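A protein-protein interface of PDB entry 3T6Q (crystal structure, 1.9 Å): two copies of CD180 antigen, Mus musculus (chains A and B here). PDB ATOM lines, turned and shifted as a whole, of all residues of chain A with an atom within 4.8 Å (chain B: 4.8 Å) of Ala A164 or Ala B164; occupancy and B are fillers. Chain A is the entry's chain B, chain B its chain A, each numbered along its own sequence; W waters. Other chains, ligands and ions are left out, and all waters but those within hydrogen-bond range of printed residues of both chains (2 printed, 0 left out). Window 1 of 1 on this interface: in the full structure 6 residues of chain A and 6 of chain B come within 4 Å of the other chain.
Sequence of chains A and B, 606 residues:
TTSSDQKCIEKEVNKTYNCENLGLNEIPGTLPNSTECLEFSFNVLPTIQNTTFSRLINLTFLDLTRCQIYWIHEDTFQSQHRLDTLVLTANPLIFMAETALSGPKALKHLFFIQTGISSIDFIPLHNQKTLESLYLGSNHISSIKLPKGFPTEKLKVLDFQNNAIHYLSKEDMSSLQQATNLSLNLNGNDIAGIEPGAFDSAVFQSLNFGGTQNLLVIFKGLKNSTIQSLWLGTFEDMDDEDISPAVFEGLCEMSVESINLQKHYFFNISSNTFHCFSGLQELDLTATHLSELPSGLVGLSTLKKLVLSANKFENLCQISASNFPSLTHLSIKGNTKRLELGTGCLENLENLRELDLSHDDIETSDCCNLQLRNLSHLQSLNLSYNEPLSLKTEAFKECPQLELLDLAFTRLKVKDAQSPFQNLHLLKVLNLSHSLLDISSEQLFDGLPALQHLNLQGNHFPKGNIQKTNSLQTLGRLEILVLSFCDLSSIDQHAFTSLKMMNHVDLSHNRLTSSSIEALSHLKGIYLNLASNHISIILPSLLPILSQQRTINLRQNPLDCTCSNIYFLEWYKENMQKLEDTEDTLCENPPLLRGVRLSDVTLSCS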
ATOM      1  N   HIS A 140     -22.734 -15.184 -27.038  1.00  0.00           N
ATOM      2  CA  HIS A 140     -23.455 -14.259 -26.161  1.00  0.00           C
ATOM      3  C   HIS A 140     -24.945 -14.525 -26.154  1.00  0.00           C
ATOM      4  O   HIS A 140     -25.740 -13.647 -25.807  1.00  0.00           O
ATOM      5  CB  HIS A 140     -23.213 -12.826 -26.604  1.00  0.00           C
ATOM      6  CG  HIS A 140     -21.762 -12.385 -26.537  1.00  0.00           C
ATOM      7  ND1 HIS A 140     -21.205 -11.885 -25.410  1.00  0.00           N
ATOM      8  CD2 HIS A 140     -20.783 -12.318 -27.517  1.00  0.00           C
ATOM      9  CE1 HIS A 140     -19.927 -11.544 -25.657  1.00  0.00           C
ATOM     10  NE2 HIS A 140     -19.671 -11.811 -26.947  1.00  0.00           N
ATOM     11  N   ILE A 141     -25.362 -15.725 -26.521  1.00  0.00           N
ATOM     12  CA  ILE A 141     -26.791 -16.007 -26.705  1.00  0.00           C
ATOM     13  C   ILE A 141     -27.580 -16.021 -25.381  1.00  0.00           C
ATOM     14  O   ILE A 141     -27.112 -16.593 -24.413  1.00  0.00           O
ATOM     15  CB  ILE A 141     -26.978 -17.341 -27.484  1.00  0.00           C
ATOM     16  CG1 ILE A 141     -26.455 -17.193 -28.929  1.00  0.00           C
ATOM     17  CG2 ILE A 141     -28.438 -17.797 -27.478  1.00  0.00           C
ATOM     18  CD1 ILE A 141     -26.100 -18.530 -29.573  1.00  0.00           C
ATOM     19  N   SER A 142     -28.787 -15.421 -25.355  1.00  0.00           N
ATOM     20  CA  SER A 142     -29.598 -15.399 -24.120  1.00  0.00           C
ATOM     21  C   SER A 142     -30.981 -16.045 -24.273  1.00  0.00           C
ATOM     22  O   SER A 142     -31.762 -16.074 -23.339  1.00  0.00           O
ATOM     23  CB  SER A 142     -29.723 -13.963 -23.585  1.00  0.00           C
ATOM     24  OG  SER A 142     -30.262 -13.125 -24.588  1.00  0.00           O
ATOM     25  N   ASN A 162     -22.394 -23.076 -22.296  1.00  0.00           N
ATOM     26  CA  ASN A 162     -21.579 -21.873 -22.033  1.00  0.00           C
ATOM     27  C   ASN A 162     -22.139 -20.635 -22.745  1.00  0.00           C
ATOM     28  O   ASN A 162     -21.472 -19.977 -23.567  1.00  0.00           O
ATOM     29  CB  ASN A 162     -20.095 -22.128 -22.397  1.00  0.00           C
ATOM     30  CG  ASN A 162     -19.171 -20.980 -21.988  1.00  0.00           C
ATOM     31  OD1 ASN A 162     -19.416 -20.289 -20.996  1.00  0.00           O
ATOM     32  ND2 ASN A 162     -18.120 -20.762 -22.765  1.00  0.00           N
ATOM     33  N   ASN A 163     -23.397 -20.313 -22.448  1.00  0.00           N
ATOM     34  CA  ASN A 163     -23.974 -19.096 -23.006  1.00  0.00           C
ATOM     35  C   ASN A 163     -24.544 -18.224 -21.869  1.00  0.00           C
ATOM     36  O   ASN A 163     -24.198 -18.406 -20.702  1.00  0.00           O
ATOM     37  CB  ASN A 163     -25.024 -19.460 -24.082  1.00  0.00           C
ATOM     38  CG  ASN A 163     -24.429 -19.514 -25.475  1.00  0.00           C
ATOM     39  OD1 ASN A 163     -24.011 -18.512 -26.006  1.00  0.00           O
ATOM     40  ND2 ASN A 163     -24.449 -20.691 -26.087  1.00  0.00           N
ATOM     41  N   ALA A 164     -25.393 -17.274 -22.222  1.00  0.00           N
ATOM     42  CA  ALA A 164     -25.960 -16.347 -21.248  1.00  0.00           C
ATOM     43  C   ALA A 164     -27.483 -16.541 -21.138  1.00  0.00           C
ATOM     44  O   ALA A 164     -28.230 -15.570 -21.028  1.00  0.00           O
ATOM     45  CB  ALA A 164     -25.623 -14.920 -21.665  1.00  0.00           C
ATOM     46  N   ILE A 165     -27.931 -17.794 -21.172  1.00  0.00           N
ATOM     47  CA  ILE A 165     -29.369 -18.126 -21.032  1.00  0.00           C
ATOM     48  C   ILE A 165     -29.788 -18.256 -19.561  1.00  0.00           C
ATOM     49  O   ILE A 165     -29.310 -19.111 -18.837  1.00  0.00           O
ATOM     50  CB  ILE A 165     -29.755 -19.365 -21.863  1.00  0.00           C
ATOM     51  CG1 ILE A 165     -29.488 -19.099 -23.363  1.00  0.00           C
ATOM     52  CG2 ILE A 165     -31.219 -19.763 -21.637  1.00  0.00           C
ATOM     53  CD1 ILE A 165     -29.161 -20.385 -24.136  1.00  0.00           C
ATOM     54  N   HIS A 166     -30.699 -17.389 -19.114  1.00  0.00           N
ATOM     55  CA  HIS A 166     -31.127 -17.461 -17.721  1.00  0.00           C
ATOM     56  C   HIS A 166     -32.607 -17.692 -17.576  1.00  0.00           C
ATOM     57  O   HIS A 166     -33.081 -17.931 -16.474  1.00  0.00           O
ATOM     58  CB  HIS A 166     -30.705 -16.218 -16.956  1.00  0.00           C
ATOM     59  CG  HIS A 166     -31.444 -14.963 -17.370  1.00  0.00           C
ATOM     60  ND1 HIS A 166     -31.023 -14.166 -18.384  1.00  0.00           N
ATOM     61  CD2 HIS A 166     -32.615 -14.364 -16.857  1.00  0.00           C
ATOM     62  CE1 HIS A 166     -31.871 -13.114 -18.515  1.00  0.00           C
ATOM     63  NE2 HIS A 166     -32.839 -13.232 -17.573  1.00  0.00           N
ATOM     64  N   ASN A 189     -25.222 -22.719 -18.413  1.00  0.00           N
ATOM     65  CA  ASN A 189     -26.183 -21.594 -18.441  1.00  0.00           C
ATOM     66  C   ASN A 189     -26.920 -21.596 -17.100  1.00  0.00           C
ATOM     67  O   ASN A 189     -27.647 -22.541 -16.785  1.00  0.00           O
ATOM     68  CB  ASN A 189     -27.201 -21.730 -19.582  1.00  0.00           C
ATOM     69  CG  ASN A 189     -26.574 -21.556 -20.951  1.00  0.00           C
ATOM     70  OD1 ASN A 189     -26.501 -20.438 -21.465  1.00  0.00           O
ATOM     71  ND2 ASN A 189     -26.066 -22.655 -21.528  1.00  0.00           N
ATOM     72  N   HIS B 140     -18.361 -10.970 -21.534  1.00  0.00           N
ATOM     73  CA  HIS B 140     -19.207 -12.107 -21.139  1.00  0.00           C
ATOM     74  C   HIS B 140     -19.407 -12.085 -19.632  1.00  0.00           C
ATOM     75  O   HIS B 140     -19.639 -13.127 -18.994  1.00  0.00           O
ATOM     76  CB  HIS B 140     -18.558 -13.482 -21.490  1.00  0.00           C
ATOM     77  CG  HIS B 140     -18.348 -13.734 -22.969  1.00  0.00           C
ATOM     78  ND1 HIS B 140     -19.303 -14.274 -23.763  1.00  0.00           N
ATOM     79  CD2 HIS B 140     -17.222 -13.543 -23.782  1.00  0.00           C
ATOM     80  CE1 HIS B 140     -18.825 -14.397 -25.021  1.00  0.00           C
ATOM     81  NE2 HIS B 140     -17.552 -13.950 -25.034  1.00  0.00           N
ATOM     82  N   ILE B 141     -19.277 -10.919 -19.039  1.00  0.00           N
ATOM     83  CA  ILE B 141     -19.252 -10.796 -17.566  1.00  0.00           C
ATOM     84  C   ILE B 141     -20.667 -11.039 -17.045  1.00  0.00           C
ATOM     85  O   ILE B 141     -21.658 -10.510 -17.610  1.00  0.00           O
ATOM     86  CB  ILE B 141     -18.747  -9.380 -17.166  1.00  0.00           C
ATOM     87  CG1 ILE B 141     -17.262  -9.241 -17.535  1.00  0.00           C
ATOM     88  CG2 ILE B 141     -18.896  -9.107 -15.669  1.00  0.00           C
ATOM     89  CD1 ILE B 141     -16.703  -7.815 -17.455  1.00  0.00           C
ATOM     90  N   SER B 142     -20.806 -11.802 -15.963  1.00  0.00           N
ATOM     91  CA  SER B 142     -22.162 -12.037 -15.459  1.00  0.00           C
ATOM     92  C   SER B 142     -22.334 -11.638 -14.004  1.00  0.00           C
ATOM     93  O   SER B 142     -23.361 -11.880 -13.422  1.00  0.00           O
ATOM     94  CB  SER B 142     -22.571 -13.489 -15.631  1.00  0.00           C
ATOM     95  OG  SER B 142     -21.626 -14.302 -14.954  1.00  0.00           O
ATOM     96  N   ASN B 162     -23.921  -3.710 -21.934  1.00  0.00           N
ATOM     97  CA  ASN B 162     -23.872  -4.839 -22.882  1.00  0.00           C
ATOM     98  C   ASN B 162     -23.108  -6.084 -22.364  1.00  0.00           C
ATOM     99  O   ASN B 162     -22.173  -6.565 -23.001  1.00  0.00           O
ATOM    100  CB  ASN B 162     -23.326  -4.374 -24.258  1.00  0.00           C
ATOM    101  CG  ASN B 162     -23.505  -5.424 -25.355  1.00  0.00           C
ATOM    102  OD1 ASN B 162     -24.486  -6.178 -25.369  1.00  0.00           O
ATOM    103  ND2 ASN B 162     -22.602  -5.432 -26.305  1.00  0.00           N
ATOM    104  N   ASN B 163     -23.528  -6.628 -21.211  1.00  0.00           N
ATOM    105  CA  ASN B 163     -22.909  -7.838 -20.659  1.00  0.00           C
ATOM    106  C   ASN B 163     -24.013  -8.837 -20.346  1.00  0.00           C
ATOM    107  O   ASN B 163     -25.113  -8.701 -20.851  1.00  0.00           O
ATOM    108  CB  ASN B 163     -22.016  -7.499 -19.440  1.00  0.00           C
ATOM    109  CG  ASN B 163     -20.576  -7.160 -19.845  1.00  0.00           C
ATOM    110  OD1 ASN B 163     -19.832  -8.035 -20.257  1.00  0.00           O
ATOM    111  ND2 ASN B 163     -20.198  -5.898 -19.766  1.00  0.00           N
ATOM    112  N   ALA B 164     -23.716  -9.858 -19.561  1.00  0.00           N
ATOM    113  CA  ALA B 164     -24.644 -10.925 -19.319  1.00  0.00           C
ATOM    114  C   ALA B 164     -25.022 -10.930 -17.850  1.00  0.00           C
ATOM    115  O   ALA B 164     -25.154 -11.989 -17.234  1.00  0.00           O
ATOM    116  CB  ALA B 164     -23.996 -12.256 -19.703  1.00  0.00           C
ATOM    117  N   ILE B 165     -25.143  -9.758 -17.253  1.00  0.00           N
ATOM    118  CA  ILE B 165     -25.498  -9.728 -15.808  1.00  0.00           C
ATOM    119  C   ILE B 165     -27.018  -9.862 -15.656  1.00  0.00           C
ATOM    120  O   ILE B 165     -27.782  -9.077 -16.229  1.00  0.00           O
ATOM    121  CB  ILE B 165     -24.981  -8.437 -15.138  1.00  0.00           C
ATOM    122  CG1 ILE B 165     -23.454  -8.413 -15.204  1.00  0.00           C
ATOM    123  CG2 ILE B 165     -25.431  -8.328 -13.658  1.00  0.00           C
ATOM    124  CD1 ILE B 165     -22.879  -7.039 -15.304  1.00  0.00           C
ATOM    125  N   HIS B 166     -27.467 -10.830 -14.857  1.00  0.00           N
ATOM    126  CA  HIS B 166     -28.889 -11.012 -14.689  1.00  0.00           C
ATOM    127  C   HIS B 166     -29.379 -10.897 -13.264  1.00  0.00           C
ATOM    128  O   HIS B 166     -30.594 -10.979 -13.023  1.00  0.00           O
ATOM    129  CB  HIS B 166     -29.358 -12.320 -15.339  1.00  0.00           C
ATOM    130  CG  HIS B 166     -28.803 -13.585 -14.702  1.00  0.00           C
ATOM    131  ND1 HIS B 166     -27.575 -14.090 -15.010  1.00  0.00           N
ATOM    132  CD2 HIS B 166     -29.382 -14.491 -13.783  1.00  0.00           C
ATOM    133  CE1 HIS B 166     -27.370 -15.239 -14.309  1.00  0.00           C
ATOM    134  NE2 HIS B 166     -28.481 -15.480 -13.562  1.00  0.00           N
ATOM    135  N   ASN B 189     -28.036  -4.917 -19.852  1.00  0.00           N
ATOM    136  CA  ASN B 189     -27.995  -6.160 -19.089  1.00  0.00           C
ATOM    137  C   ASN B 189     -29.418  -6.461 -18.615  1.00  0.00           C
ATOM    138  O   ASN B 189     -30.056  -5.636 -17.956  1.00  0.00           O
ATOM    139  CB  ASN B 189     -27.100  -5.997 -17.840  1.00  0.00           C
ATOM    140  CG  ASN B 189     -25.609  -5.934 -18.194  1.00  0.00           C
ATOM    141  OD1 ASN B 189     -24.940  -6.969 -18.257  1.00  0.00           O
ATOM    142  ND2 ASN B 189     -25.112  -4.752 -18.493  1.00  0.00           N
HETATM  143  O   HOH W   1     -20.017 -17.588 -23.618  1.00  0.00           O
HETATM  144  O   HOH W   2     -21.739  -8.851 -24.615  1.00  0.00           O
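ND1 of His B140 lies close to ND1 of His A140, at 3.5 Å.
Of the 9 printed residues of chain A, 3 touch a printed residue of chain B. Printed residues of chain B that touch a printed residue of chain A: His B140, Ala B164 and His B166.
Among the printed residues, pairs that only touch across the chains: Ala A164 with Ala B164 (3.7 Å) and His A166 with His B166 (3.8 Å).
His B140 touches its own counterpart, His A140. Ala B164 touches its own counterpart, Ala A164. His A166 touches its own counterpart, His B166. 9 positions are printed for both chains.
Ala A164 touches one residue of chain B. Of chain A, only Ala A164 comes within 4 Å of Ala B164. Printed residues of chain A within 4 Å of His B166: His A166. Of the printed residues of chain A, His B140 touches His A140 (3.1 Å). Of the printed residues of chain B, His A140 touches His B140. Asn B162 touches none of the printed residues of chain A. The nearest printed residue of chain B that does not touch Ala A164 is His B166 (6.2 Å). The nearest printed residue of chain A that does not touch Ala B164 is Asn A163 (6.2 Å). The nearest printed residue of chain B that does not touch His A166 is Ile B165 (6.2 Å).
The side-chain amide oxygen (OD1) of Asn A189 sits at hydrogen-bond distance from the backbone NH (N) of Ala A164. The backbone NH of Ala B164 sits at hydrogen-bond distance from the side-chain amide oxygen of Asn B189 (3.4 Å). The backbone NH (N) of Ala B164 sits at hydrogen-bond distance from the backbone carbonyl oxygen (O) of Ile B141 (2.9 Å). N of Ala A164 sits at hydrogen-bond distance from O of Ile A141, at 2.9 Å.
Water W1 lies within hydrogen-bond range of the backbone carbonyl oxygen of Asn A162 (2.8 Å) and a ring nitrogen (ND1) of His B140 (3.4 Å). Water W2 bridges the backbone carbonyl oxygen (O) of Asn B162 (2.8 Å) and a ring nitrogen (ND1) of His A140 (3.2 Å).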
